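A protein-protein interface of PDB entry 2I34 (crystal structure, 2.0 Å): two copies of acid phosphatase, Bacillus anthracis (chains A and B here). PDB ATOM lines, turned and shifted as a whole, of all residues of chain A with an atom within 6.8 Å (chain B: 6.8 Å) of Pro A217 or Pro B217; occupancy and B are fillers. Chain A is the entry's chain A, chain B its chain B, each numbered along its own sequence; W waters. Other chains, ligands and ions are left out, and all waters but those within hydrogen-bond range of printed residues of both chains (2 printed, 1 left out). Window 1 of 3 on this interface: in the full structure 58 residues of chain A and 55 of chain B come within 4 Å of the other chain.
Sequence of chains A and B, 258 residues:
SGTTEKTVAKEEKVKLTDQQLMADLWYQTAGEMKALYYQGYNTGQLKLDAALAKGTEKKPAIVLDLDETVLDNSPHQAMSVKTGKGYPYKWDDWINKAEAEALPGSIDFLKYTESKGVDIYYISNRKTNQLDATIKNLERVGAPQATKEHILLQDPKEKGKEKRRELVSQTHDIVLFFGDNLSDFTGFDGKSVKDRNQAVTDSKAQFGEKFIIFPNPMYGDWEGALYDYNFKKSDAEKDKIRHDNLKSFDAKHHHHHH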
ATOM      1  N   GLN A  20     -34.641  15.723 -37.451  1.00  0.00           N
ATOM      2  CA  GLN A  20     -33.757  15.291 -36.377  1.00  0.00           C
ATOM      3  C   GLN A  20     -32.304  15.187 -36.835  1.00  0.00           C
ATOM      4  O   GLN A  20     -31.417  14.932 -36.020  1.00  0.00           O
ATOM      5  CB  GLN A  20     -34.232  13.946 -35.798  1.00  0.00           C
ATOM      6  CG  GLN A  20     -33.980  12.745 -36.698  1.00  0.00           C
ATOM      7  CD  GLN A  20     -34.813  11.517 -36.340  1.00  0.00           C
ATOM      8  OE1 GLN A  20     -34.276  10.407 -36.176  1.00  0.00           O
ATOM      9  NE2 GLN A  20     -36.134  11.704 -36.226  1.00  0.00           N
ATOM     10  N   MET A  22     -29.629  17.136 -37.716  1.00  0.00           N
ATOM     11  CA  MET A  22     -28.550  17.866 -36.995  1.00  0.00           C
ATOM     12  C   MET A  22     -28.395  17.427 -35.541  1.00  0.00           C
ATOM     13  O   MET A  22     -27.278  17.225 -35.072  1.00  0.00           O
ATOM     14  CB  MET A  22     -28.756  19.386 -37.043  1.00  0.00           C
ATOM     15  CG  MET A  22     -28.499  19.981 -38.411  1.00  0.00           C
ATOM     16  SD  MET A  22     -26.755  19.864 -38.860  1.00  0.00           S
ATOM     17  CE  MET A  22     -26.158  21.430 -38.288  1.00  0.00           C
ATOM     18  N   ALA A  23     -29.511  17.284 -34.833  1.00  0.00           N
ATOM     19  CA  ALA A  23     -29.498  16.727 -33.476  1.00  0.00           C
ATOM     20  C   ALA A  23     -28.774  15.365 -33.404  1.00  0.00           C
ATOM     21  O   ALA A  23     -27.959  15.134 -32.506  1.00  0.00           O
ATOM     22  CB  ALA A  23     -30.919  16.580 -32.960  1.00  0.00           C
ATOM     23  N   ASP A  24     -29.074  14.482 -34.354  1.00  0.00           N
ATOM     24  CA  ASP A  24     -28.457  13.157 -34.403  1.00  0.00           C
ATOM     25  C   ASP A  24     -26.980  13.217 -34.722  1.00  0.00           C
ATOM     26  O   ASP A  24     -26.189  12.451 -34.169  1.00  0.00           O
ATOM     27  CB  ASP A  24     -29.134  12.285 -35.455  1.00  0.00           C
ATOM     28  CG  ASP A  24     -30.559  11.912 -35.087  1.00  0.00           C
ATOM     29  OD1 ASP A  24     -30.978  12.171 -33.934  1.00  0.00           O
ATOM     30  OD2 ASP A  24     -31.242  11.345 -35.972  1.00  0.00           O
ATOM     31  N   TRP A  26     -24.848  15.834 -34.318  1.00  0.00           N
ATOM     32  CA  TRP A  26     -24.195  16.331 -33.113  1.00  0.00           C
ATOM     33  C   TRP A  26     -23.946  15.191 -32.145  1.00  0.00           C
ATOM     34  O   TRP A  26     -22.832  14.988 -31.685  1.00  0.00           O
ATOM     35  CB  TRP A  26     -25.069  17.389 -32.413  1.00  0.00           C
ATOM     36  CG  TRP A  26     -24.412  18.018 -31.209  1.00  0.00           C
ATOM     37  CD1 TRP A  26     -23.481  19.004 -31.226  1.00  0.00           C
ATOM     38  CD2 TRP A  26     -24.646  17.714 -29.819  1.00  0.00           C
ATOM     39  NE1 TRP A  26     -23.108  19.328 -29.953  1.00  0.00           N
ATOM     40  CE2 TRP A  26     -23.823  18.570 -29.066  1.00  0.00           C
ATOM     41  CE3 TRP A  26     -25.492  16.819 -29.143  1.00  0.00           C
ATOM     42  CZ2 TRP A  26     -23.781  18.542 -27.660  1.00  0.00           C
ATOM     43  CZ3 TRP A  26     -25.458  16.786 -27.755  1.00  0.00           C
ATOM     44  CH2 TRP A  26     -24.606  17.652 -27.026  1.00  0.00           C
ATOM     45  N   TYR A  27     -24.999  14.460 -31.830  1.00  0.00           N
ATOM     46  CA  TYR A  27     -24.907  13.445 -30.808  1.00  0.00           C
ATOM     47  C   TYR A  27     -23.895  12.369 -31.207  1.00  0.00           C
ATOM     48  O   TYR A  27     -23.112  11.891 -30.385  1.00  0.00           O
ATOM     49  CB  TYR A  27     -26.280  12.847 -30.534  1.00  0.00           C
ATOM     50  CG  TYR A  27     -26.311  12.005 -29.310  1.00  0.00           C
ATOM     51  CD1 TYR A  27     -26.597  12.563 -28.082  1.00  0.00           C
ATOM     52  CD2 TYR A  27     -26.019  10.644 -29.369  1.00  0.00           C
ATOM     53  CE1 TYR A  27     -26.614  11.779 -26.924  1.00  0.00           C
ATOM     54  CE2 TYR A  27     -26.044   9.846 -28.215  1.00  0.00           C
ATOM     55  CZ  TYR A  27     -26.337  10.432 -26.995  1.00  0.00           C
ATOM     56  OH  TYR A  27     -26.365   9.689 -25.841  1.00  0.00           O
ATOM     57  N   PHE A 214     -27.522  14.574 -18.676  1.00  0.00           N
ATOM     58  CA  PHE A 214     -26.783  14.403 -19.931  1.00  0.00           C
ATOM     59  C   PHE A 214     -27.593  14.931 -21.134  1.00  0.00           C
ATOM     60  O   PHE A 214     -28.830  14.897 -21.103  1.00  0.00           O
ATOM     61  CB  PHE A 214     -26.451  12.922 -20.131  1.00  0.00           C
ATOM     62  CG  PHE A 214     -25.500  12.392 -19.109  1.00  0.00           C
ATOM     63  CD1 PHE A 214     -24.134  12.660 -19.213  1.00  0.00           C
ATOM     64  CD2 PHE A 214     -25.959  11.669 -18.026  1.00  0.00           C
ATOM     65  CE1 PHE A 214     -23.254  12.200 -18.268  1.00  0.00           C
ATOM     66  CE2 PHE A 214     -25.072  11.208 -17.059  1.00  0.00           C
ATOM     67  CZ  PHE A 214     -23.709  11.477 -17.189  1.00  0.00           C
ATOM     68  N   PRO A 215     -26.894  15.432 -22.189  1.00  0.00           N
ATOM     69  CA  PRO A 215     -27.582  16.039 -23.338  1.00  0.00           C
ATOM     70  C   PRO A 215     -28.156  15.049 -24.377  1.00  0.00           C
ATOM     71  O   PRO A 215     -27.422  14.221 -24.930  1.00  0.00           O
ATOM     72  CB  PRO A 215     -26.486  16.898 -23.978  1.00  0.00           C
ATOM     73  CG  PRO A 215     -25.203  16.123 -23.689  1.00  0.00           C
ATOM     74  CD  PRO A 215     -25.422  15.512 -22.323  1.00  0.00           C
ATOM     75  N   ASN A 216     -29.459  15.155 -24.643  1.00  0.00           N
ATOM     76  CA  ASN A 216     -30.114  14.353 -25.681  1.00  0.00           C
ATOM     77  C   ASN A 216     -31.112  15.198 -26.459  1.00  0.00           C
ATOM     78  O   ASN A 216     -32.293  15.245 -26.118  1.00  0.00           O
ATOM     79  CB  ASN A 216     -30.789  13.113 -25.085  1.00  0.00           C
ATOM     80  CG  ASN A 216     -31.520  12.274 -26.119  1.00  0.00           C
ATOM     81  OD1 ASN A 216     -31.431  12.518 -27.309  1.00  0.00           O
ATOM     82  ND2 ASN A 216     -32.254  11.282 -25.657  1.00  0.00           N
ATOM     83  N   PRO A 217     -30.642  15.864 -27.525  1.00  0.00           N
ATOM     84  CA  PRO A 217     -31.581  16.618 -28.374  1.00  0.00           C
ATOM     85  C   PRO A 217     -32.322  15.777 -29.436  1.00  0.00           C
ATOM     86  O   PRO A 217     -33.031  16.345 -30.265  1.00  0.00           O
ATOM     87  CB  PRO A 217     -30.664  17.637 -29.041  1.00  0.00           C
ATOM     88  CG  PRO A 217     -29.370  16.853 -29.225  1.00  0.00           C
ATOM     89  CD  PRO A 217     -29.251  15.998 -27.991  1.00  0.00           C
ATOM     90  N   MET A 218     -32.168  14.447 -29.404  1.00  0.00           N
ATOM     91  CA  MET A 218     -32.754  13.561 -30.416  1.00  0.00           C
ATOM     92  C   MET A 218     -34.222  13.218 -30.112  1.00  0.00           C
ATOM     93  O   MET A 218     -35.060  13.193 -31.010  1.00  0.00           O
ATOM     94  CB  MET A 218     -31.954  12.261 -30.515  1.00  0.00           C
ATOM     95  CG  MET A 218     -30.465  12.446 -30.785  1.00  0.00           C
ATOM     96  SD  MET A 218     -29.608  10.886 -31.032  1.00  0.00           S
ATOM     97  CE  MET A 218     -29.702  10.194 -29.365  1.00  0.00           C
ATOM     98  N   TYR A 219     -34.515  12.956 -28.840  1.00  0.00           N
ATOM     99  CA  TYR A 219     -35.815  12.470 -28.425  1.00  0.00           C
ATOM    100  C   TYR A 219     -35.977  12.612 -26.907  1.00  0.00           C
ATOM    101  O   TYR A 219     -35.012  12.904 -26.197  1.00  0.00           O
ATOM    102  CB  TYR A 219     -35.987  10.998 -28.855  1.00  0.00           C
ATOM    103  CG  TYR A 219     -35.151  10.029 -28.037  1.00  0.00           C
ATOM    104  CD1 TYR A 219     -33.863   9.674 -28.418  1.00  0.00           C
ATOM    105  CD2 TYR A 219     -35.654   9.502 -26.851  1.00  0.00           C
ATOM    106  CE1 TYR A 219     -33.112   8.801 -27.645  1.00  0.00           C
ATOM    107  CE2 TYR A 219     -34.909   8.640 -26.073  1.00  0.00           C
ATOM    108  CZ  TYR A 219     -33.644   8.291 -26.459  1.00  0.00           C
ATOM    109  OH  TYR A 219     -32.937   7.423 -25.634  1.00  0.00           O
ATOM    110  N   GLY A 220     -37.197  12.394 -26.422  1.00  0.00           N
ATOM    111  CA  GLY A 220     -37.451  12.280 -24.983  1.00  0.00           C
ATOM    112  C   GLY A 220     -38.749  12.916 -24.553  1.00  0.00           C
ATOM    113  O   GLY A 220     -39.551  13.303 -25.397  1.00  0.00           O
ATOM    114  N   TRP A 222     -39.111  15.822 -23.404  1.00  0.00           N
ATOM    115  CA  TRP A 222     -39.168  17.201 -23.920  1.00  0.00           C
ATOM    116  C   TRP A 222     -40.009  17.288 -25.199  1.00  0.00           C
ATOM    117  O   TRP A 222     -40.706  18.294 -25.435  1.00  0.00           O
ATOM    118  CB  TRP A 222     -37.754  17.766 -24.156  1.00  0.00           C
ATOM    119  CG  TRP A 222     -37.014  17.170 -25.314  1.00  0.00           C
ATOM    120  CD1 TRP A 222     -36.157  16.118 -25.277  1.00  0.00           C
ATOM    121  CD2 TRP A 222     -37.051  17.612 -26.681  1.00  0.00           C
ATOM    122  NE1 TRP A 222     -35.664  15.863 -26.531  1.00  0.00           N
ATOM    123  CE2 TRP A 222     -36.206  16.757 -27.414  1.00  0.00           C
ATOM    124  CE3 TRP A 222     -37.731  18.643 -27.356  1.00  0.00           C
ATOM    125  CZ2 TRP A 222     -35.997  16.906 -28.786  1.00  0.00           C
ATOM    126  CZ3 TRP A 222     -37.546  18.781 -28.719  1.00  0.00           C
ATOM    127  CH2 TRP A 222     -36.693  17.913 -29.426  1.00  0.00           C
ATOM    128  N   GLN B  20     -32.251  21.369 -38.927  1.00  0.00           N
ATOM    129  CA  GLN B  20     -31.941  21.979 -37.630  1.00  0.00           C
ATOM    130  C   GLN B  20     -33.129  22.002 -36.660  1.00  0.00           C
ATOM    131  O   GLN B  20     -32.942  22.331 -35.497  1.00  0.00           O
ATOM    132  CB  GLN B  20     -31.438  23.413 -37.805  1.00  0.00           C
ATOM    133  CG  GLN B  20     -30.473  23.873 -36.684  1.00  0.00           C
ATOM    134  CD  GLN B  20     -30.209  25.380 -36.679  1.00  0.00           C
ATOM    135  OE1 GLN B  20     -31.089  26.193 -36.991  1.00  0.00           O
ATOM    136  NE2 GLN B  20     -28.992  25.754 -36.313  1.00  0.00           N
ATOM    137  N   MET B  22     -35.250  20.016 -34.813  1.00  0.00           N
ATOM    138  CA  MET B  22     -35.293  19.339 -33.509  1.00  0.00           C
ATOM    139  C   MET B  22     -34.227  19.856 -32.551  1.00  0.00           C
ATOM    140  O   MET B  22     -34.499  20.039 -31.358  1.00  0.00           O
ATOM    141  CB  MET B  22     -35.208  17.816 -33.667  1.00  0.00           C
ATOM    142  CG  MET B  22     -36.499  17.199 -34.212  1.00  0.00           C
ATOM    143  SD  MET B  22     -37.881  17.325 -33.042  1.00  0.00           S
ATOM    144  CE  MET B  22     -37.497  15.950 -31.966  1.00  0.00           C
ATOM    145  N   ALA B  23     -33.022  20.094 -33.075  1.00  0.00           N
ATOM    146  CA  ALA B  23     -31.943  20.717 -32.320  1.00  0.00           C
ATOM    147  C   ALA B  23     -32.363  22.062 -31.713  1.00  0.00           C
ATOM    148  O   ALA B  23     -32.093  22.314 -30.525  1.00  0.00           O
ATOM    149  CB  ALA B  23     -30.703  20.902 -33.201  1.00  0.00           C
ATOM    150  N   ASP B  24     -33.012  22.911 -32.524  1.00  0.00           N
ATOM    151  CA  ASP B  24     -33.497  24.240 -32.066  1.00  0.00           C
ATOM    152  C   ASP B  24     -34.630  24.108 -31.068  1.00  0.00           C
ATOM    153  O   ASP B  24     -34.657  24.813 -30.068  1.00  0.00           O
ATOM    154  CB  ASP B  24     -33.993  25.127 -33.230  1.00  0.00           C
ATOM    155  CG  ASP B  24     -32.883  25.562 -34.173  1.00  0.00           C
ATOM    156  OD1 ASP B  24     -31.704  25.366 -33.835  1.00  0.00           O
ATOM    157  OD2 ASP B  24     -33.201  26.087 -35.276  1.00  0.00           O
ATOM    158  N   TRP B  26     -35.420  21.551 -29.007  1.00  0.00           N
ATOM    159  CA  TRP B  26     -34.806  21.120 -27.742  1.00  0.00           C
ATOM    160  C   TRP B  26     -34.140  22.293 -26.988  1.00  0.00           C
ATOM    161  O   TRP B  26     -34.377  22.504 -25.784  1.00  0.00           O
ATOM    162  CB  TRP B  26     -33.760  20.028 -27.998  1.00  0.00           C
ATOM    163  CG  TRP B  26     -33.103  19.521 -26.737  1.00  0.00           C
ATOM    164  CD1 TRP B  26     -33.616  18.601 -25.876  1.00  0.00           C
ATOM    165  CD2 TRP B  26     -31.835  19.918 -26.184  1.00  0.00           C
ATOM    166  NE1 TRP B  26     -32.762  18.401 -24.823  1.00  0.00           N
ATOM    167  CE2 TRP B  26     -31.657  19.191 -24.985  1.00  0.00           C
ATOM    168  CE3 TRP B  26     -30.838  20.822 -26.576  1.00  0.00           C
ATOM    169  CZ2 TRP B  26     -30.520  19.326 -24.180  1.00  0.00           C
ATOM    170  CZ3 TRP B  26     -29.704  20.953 -25.780  1.00  0.00           C
ATOM    171  CH2 TRP B  26     -29.549  20.190 -24.599  1.00  0.00           C
ATOM    172  N   TYR B  27     -33.311  23.048 -27.697  1.00  0.00           N
ATOM    173  CA  TYR B  27     -32.561  24.134 -27.073  1.00  0.00           C
ATOM    174  C   TYR B  27     -33.501  25.209 -26.518  1.00  0.00           C
ATOM    175  O   TYR B  27     -33.293  25.725 -25.409  1.00  0.00           O
ATOM    176  CB  TYR B  27     -31.580  24.745 -28.068  1.00  0.00           C
ATOM    177  CG  TYR B  27     -30.540  25.623 -27.424  1.00  0.00           C
ATOM    178  CD1 TYR B  27     -29.336  25.093 -26.974  1.00  0.00           C
ATOM    179  CD2 TYR B  27     -30.760  26.978 -27.262  1.00  0.00           C
ATOM    180  CE1 TYR B  27     -28.373  25.903 -26.379  1.00  0.00           C
ATOM    181  CE2 TYR B  27     -29.806  27.796 -26.654  1.00  0.00           C
ATOM    182  CZ  TYR B  27     -28.616  27.256 -26.229  1.00  0.00           C
ATOM    183  OH  TYR B  27     -27.670  28.049 -25.633  1.00  0.00           O
ATOM    184  N   PHE B 214     -21.165  23.500 -22.294  1.00  0.00           N
ATOM    185  CA  PHE B 214     -22.600  23.632 -22.407  1.00  0.00           C
ATOM    186  C   PHE B 214     -23.051  23.051 -23.760  1.00  0.00           C
ATOM    187  O   PHE B 214     -22.258  23.020 -24.729  1.00  0.00           O
ATOM    188  CB  PHE B 214     -22.988  25.113 -22.290  1.00  0.00           C
ATOM    189  CG  PHE B 214     -22.723  25.687 -20.936  1.00  0.00           C
ATOM    190  CD1 PHE B 214     -23.582  25.407 -19.872  1.00  0.00           C
ATOM    191  CD2 PHE B 214     -21.607  26.477 -20.702  1.00  0.00           C
ATOM    192  CE1 PHE B 214     -23.329  25.910 -18.602  1.00  0.00           C
ATOM    193  CE2 PHE B 214     -21.353  26.997 -19.423  1.00  0.00           C
ATOM    194  CZ  PHE B 214     -22.219  26.706 -18.377  1.00  0.00           C
ATOM    195  N   PRO B 215     -24.292  22.558 -23.818  1.00  0.00           N
ATOM    196  CA  PRO B 215     -24.801  21.846 -24.990  1.00  0.00           C
ATOM    197  C   PRO B 215     -25.367  22.735 -26.079  1.00  0.00           C
ATOM    198  O   PRO B 215     -26.296  23.501 -25.828  1.00  0.00           O
ATOM    199  CB  PRO B 215     -25.917  20.976 -24.402  1.00  0.00           C
ATOM    200  CG  PRO B 215     -26.412  21.768 -23.233  1.00  0.00           C
ATOM    201  CD  PRO B 215     -25.277  22.568 -22.712  1.00  0.00           C
ATOM    202  N   ASN B 216     -24.828  22.615 -27.288  1.00  0.00           N
ATOM    203  CA  ASN B 216     -25.338  23.378 -28.427  1.00  0.00           C
ATOM    204  C   ASN B 216     -25.372  22.509 -29.675  1.00  0.00           C
ATOM    205  O   ASN B 216     -24.413  22.493 -30.455  1.00  0.00           O
ATOM    206  CB  ASN B 216     -24.491  24.632 -28.664  1.00  0.00           C
ATOM    207  CG  ASN B 216     -24.953  25.430 -29.865  1.00  0.00           C
ATOM    208  OD1 ASN B 216     -26.000  25.133 -30.448  1.00  0.00           O
ATOM    209  ND2 ASN B 216     -24.167  26.431 -30.255  1.00  0.00           N
ATOM    210  N   PRO B 217     -26.488  21.789 -29.878  1.00  0.00           N
ATOM    211  CA  PRO B 217     -26.658  20.970 -31.087  1.00  0.00           C
ATOM    212  C   PRO B 217     -27.090  21.754 -32.333  1.00  0.00           C
ATOM    213  O   PRO B 217     -27.314  21.148 -33.381  1.00  0.00           O
ATOM    214  CB  PRO B 217     -27.749  19.986 -30.676  1.00  0.00           C
ATOM    215  CG  PRO B 217     -28.597  20.787 -29.683  1.00  0.00           C
ATOM    216  CD  PRO B 217     -27.639  21.673 -28.954  1.00  0.00           C
ATOM    217  N   MET B 218     -27.193  23.079 -32.228  1.00  0.00           N
ATOM    218  CA  MET B 218     -27.683  23.901 -33.314  1.00  0.00           C
ATOM    219  C   MET B 218     -26.605  24.231 -34.348  1.00  0.00           C
ATOM    220  O   MET B 218     -26.887  24.251 -35.545  1.00  0.00           O
ATOM    221  CB  MET B 218     -28.277  25.207 -32.782  1.00  0.00           C
ATOM    222  CG  MET B 218     -29.379  25.034 -31.724  1.00  0.00           C
ATOM    223  SD  MET B 218     -30.104  26.636 -31.287  1.00  0.00           S
ATOM    224  CE  MET B 218     -28.782  27.392 -30.349  1.00  0.00           C
ATOM    225  N   TYR B 219     -25.389  24.516 -33.891  1.00  0.00           N
ATOM    226  CA  TYR B 219     -24.303  24.963 -34.773  1.00  0.00           C
ATOM    227  C   TYR B 219     -22.965  24.908 -34.028  1.00  0.00           C
ATOM    228  O   TYR B 219     -22.937  24.787 -32.799  1.00  0.00           O
ATOM    229  CB  TYR B 219     -24.559  26.401 -35.290  1.00  0.00           C
ATOM    230  CG  TYR B 219     -24.364  27.440 -34.211  1.00  0.00           C
ATOM    231  CD1 TYR B 219     -23.095  27.948 -33.932  1.00  0.00           C
ATOM    232  CD2 TYR B 219     -25.436  27.884 -33.433  1.00  0.00           C
ATOM    233  CE1 TYR B 219     -22.899  28.873 -32.918  1.00  0.00           C
ATOM    234  CE2 TYR B 219     -25.251  28.821 -32.415  1.00  0.00           C
ATOM    235  CZ  TYR B 219     -23.987  29.301 -32.153  1.00  0.00           C
ATOM    236  OH  TYR B 219     -23.786  30.207 -31.129  1.00  0.00           O
ATOM    237  N   GLY B 220     -21.862  25.009 -34.773  1.00  0.00           N
ATOM    238  CA  GLY B 220     -20.532  25.165 -34.165  1.00  0.00           C
ATOM    239  C   GLY B 220     -19.397  24.537 -34.961  1.00  0.00           C
ATOM    240  O   GLY B 220     -19.564  24.148 -36.127  1.00  0.00           O
ATOM    241  N   TRP B 222     -18.236  21.705 -34.435  1.00  0.00           N
ATOM    242  CA  TRP B 222     -18.593  20.309 -34.697  1.00  0.00           C
ATOM    243  C   TRP B 222     -19.105  20.128 -36.138  1.00  0.00           C
ATOM    244  O   TRP B 222     -18.800  19.125 -36.798  1.00  0.00           O
ATOM    245  CB  TRP B 222     -19.599  19.779 -33.674  1.00  0.00           C
ATOM    246  CG  TRP B 222     -20.972  20.346 -33.748  1.00  0.00           C
ATOM    247  CD1 TRP B 222     -21.459  21.413 -33.042  1.00  0.00           C
ATOM    248  CD2 TRP B 222     -22.057  19.866 -34.551  1.00  0.00           C
ATOM    249  NE1 TRP B 222     -22.778  21.621 -33.358  1.00  0.00           N
ATOM    250  CE2 TRP B 222     -23.168  20.686 -34.284  1.00  0.00           C
ATOM    251  CE3 TRP B 222     -22.197  18.809 -35.468  1.00  0.00           C
ATOM    252  CZ2 TRP B 222     -24.412  20.483 -34.889  1.00  0.00           C
ATOM    253  CZ3 TRP B 222     -23.422  18.618 -36.081  1.00  0.00           C
ATOM    254  CH2 TRP B 222     -24.518  19.448 -35.783  1.00  0.00           C
HETATM  255  O   HOH W   1     -21.729  22.072 -29.896  1.00  0.00           O
HETATM  256  O   HOH W   2     -33.193  15.617 -23.634  1.00  0.00           O
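The backbone carbonyl oxygen (O) of Asn B216 sits at hydrogen-bond distance from the indole nitrogen (NE1) of Trp B222, 3.4 Å away.
OD2 of Asp A24 sits close to OE1 of Gln A20, at 3.2 Å.
The side-chain amide oxygen of Asn A216 sits at hydrogen-bond distance from the backbone NH of Met A218 (2.9 Å).
The backbone carbonyl oxygen of Asn A216 is in hydrogen-bond range of the indole nitrogen of Trp A222 (3.5 Å).
O of Tyr A219 is in hydrogen-bond range of NE1 of Trp A222 (3.0 Å).
The side-chain amide nitrogen (ND2) of Asn B216 sits at hydrogen-bond distance from the backbone carbonyl oxygen (O) of Tyr B219 (3.3 Å).
Water W2 bridges O of Asn A216 (2.7 Å) and NE1 of Trp B26 (3.1 Å).
Water W1 bridges O of Asn B216 (2.8 Å) and NE1 of Trp A26 (3.1 Å).
Gln A20 touches Met B22.
Trp B222 touches Met A22.
CG of Trp A26 touches CA of Pro B217 (3.7 Å).
CD1 of Trp A26 touches NE1 of Trp B222 (3.4 Å).
Pro A217 touches Trp B26.
CB of Pro B217 touches CG of Pro A217 (3.8 Å).
Met A218 touches Met B22 (O to CE, 3.8 Å).
CH2 of Trp A222 touches CE of Met B22 (3.3 Å).
Trp B26 touches Trp A222 (CD1 to NE1, 3.5 Å).
Printed residues of chain B that touch a printed residue of chain A: Met B22, Trp B26, Asn B216, Pro B217 and Trp B222.
Hydrophobic or aromatic side chains of chain B that line the printed part of chain A: Met B22, Trp B26, Pro B217 and Trp B222.
Of the 14 printed residues of chain A, 7 touch a printed residue of chain B.
Hydrophobic or aromatic side chains of chain A within 4 Å of the printed part of chain B: Met A22, Trp A26, Pro A217 and Trp A222.
NE1 of Trp A26 is in hydrogen-bond range of O of Asn B216, at 3.5 Å.
The backbone carbonyl oxygen (O) of Asn A216 sits at hydrogen-bond distance from the indole nitrogen (NE1) of Trp B26 (3.4 Å).
Of the printed residues of chain B, Met A22 touches Trp B222 (3.6 Å).
Of the printed residues of chain B, Gln A20 touches Met B22.
Of the printed residues of chain A, Trp B222 touches Met A22 (3.6 Å) and Trp A26 (3.4 Å).
Printed residues of chain A within 4 Å of Trp B26: Asn A216 (3.4 Å), Pro A217 (3.7 Å) and Trp A222 (3.5 Å).
Pro B215 touches none of the printed residues of chain A.
Met A22 touches Trp B222, and with the chains exchanged Trp A222 touches Met B22.
Trp A26 touches Asn B216, and with the chains exchanged Asn A216 touches Trp B26.
Trp A26 touches Trp B222, and with the chains exchanged Trp A222 touches Trp B26.
Met A218 touches Met B22, but with the chains exchanged Met A22 does not touch Met B218 (4.002 Å).
Of the 11 pairs that touch across the chains among the printed residues, 9 have their exchanged pair printed and touching as well.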
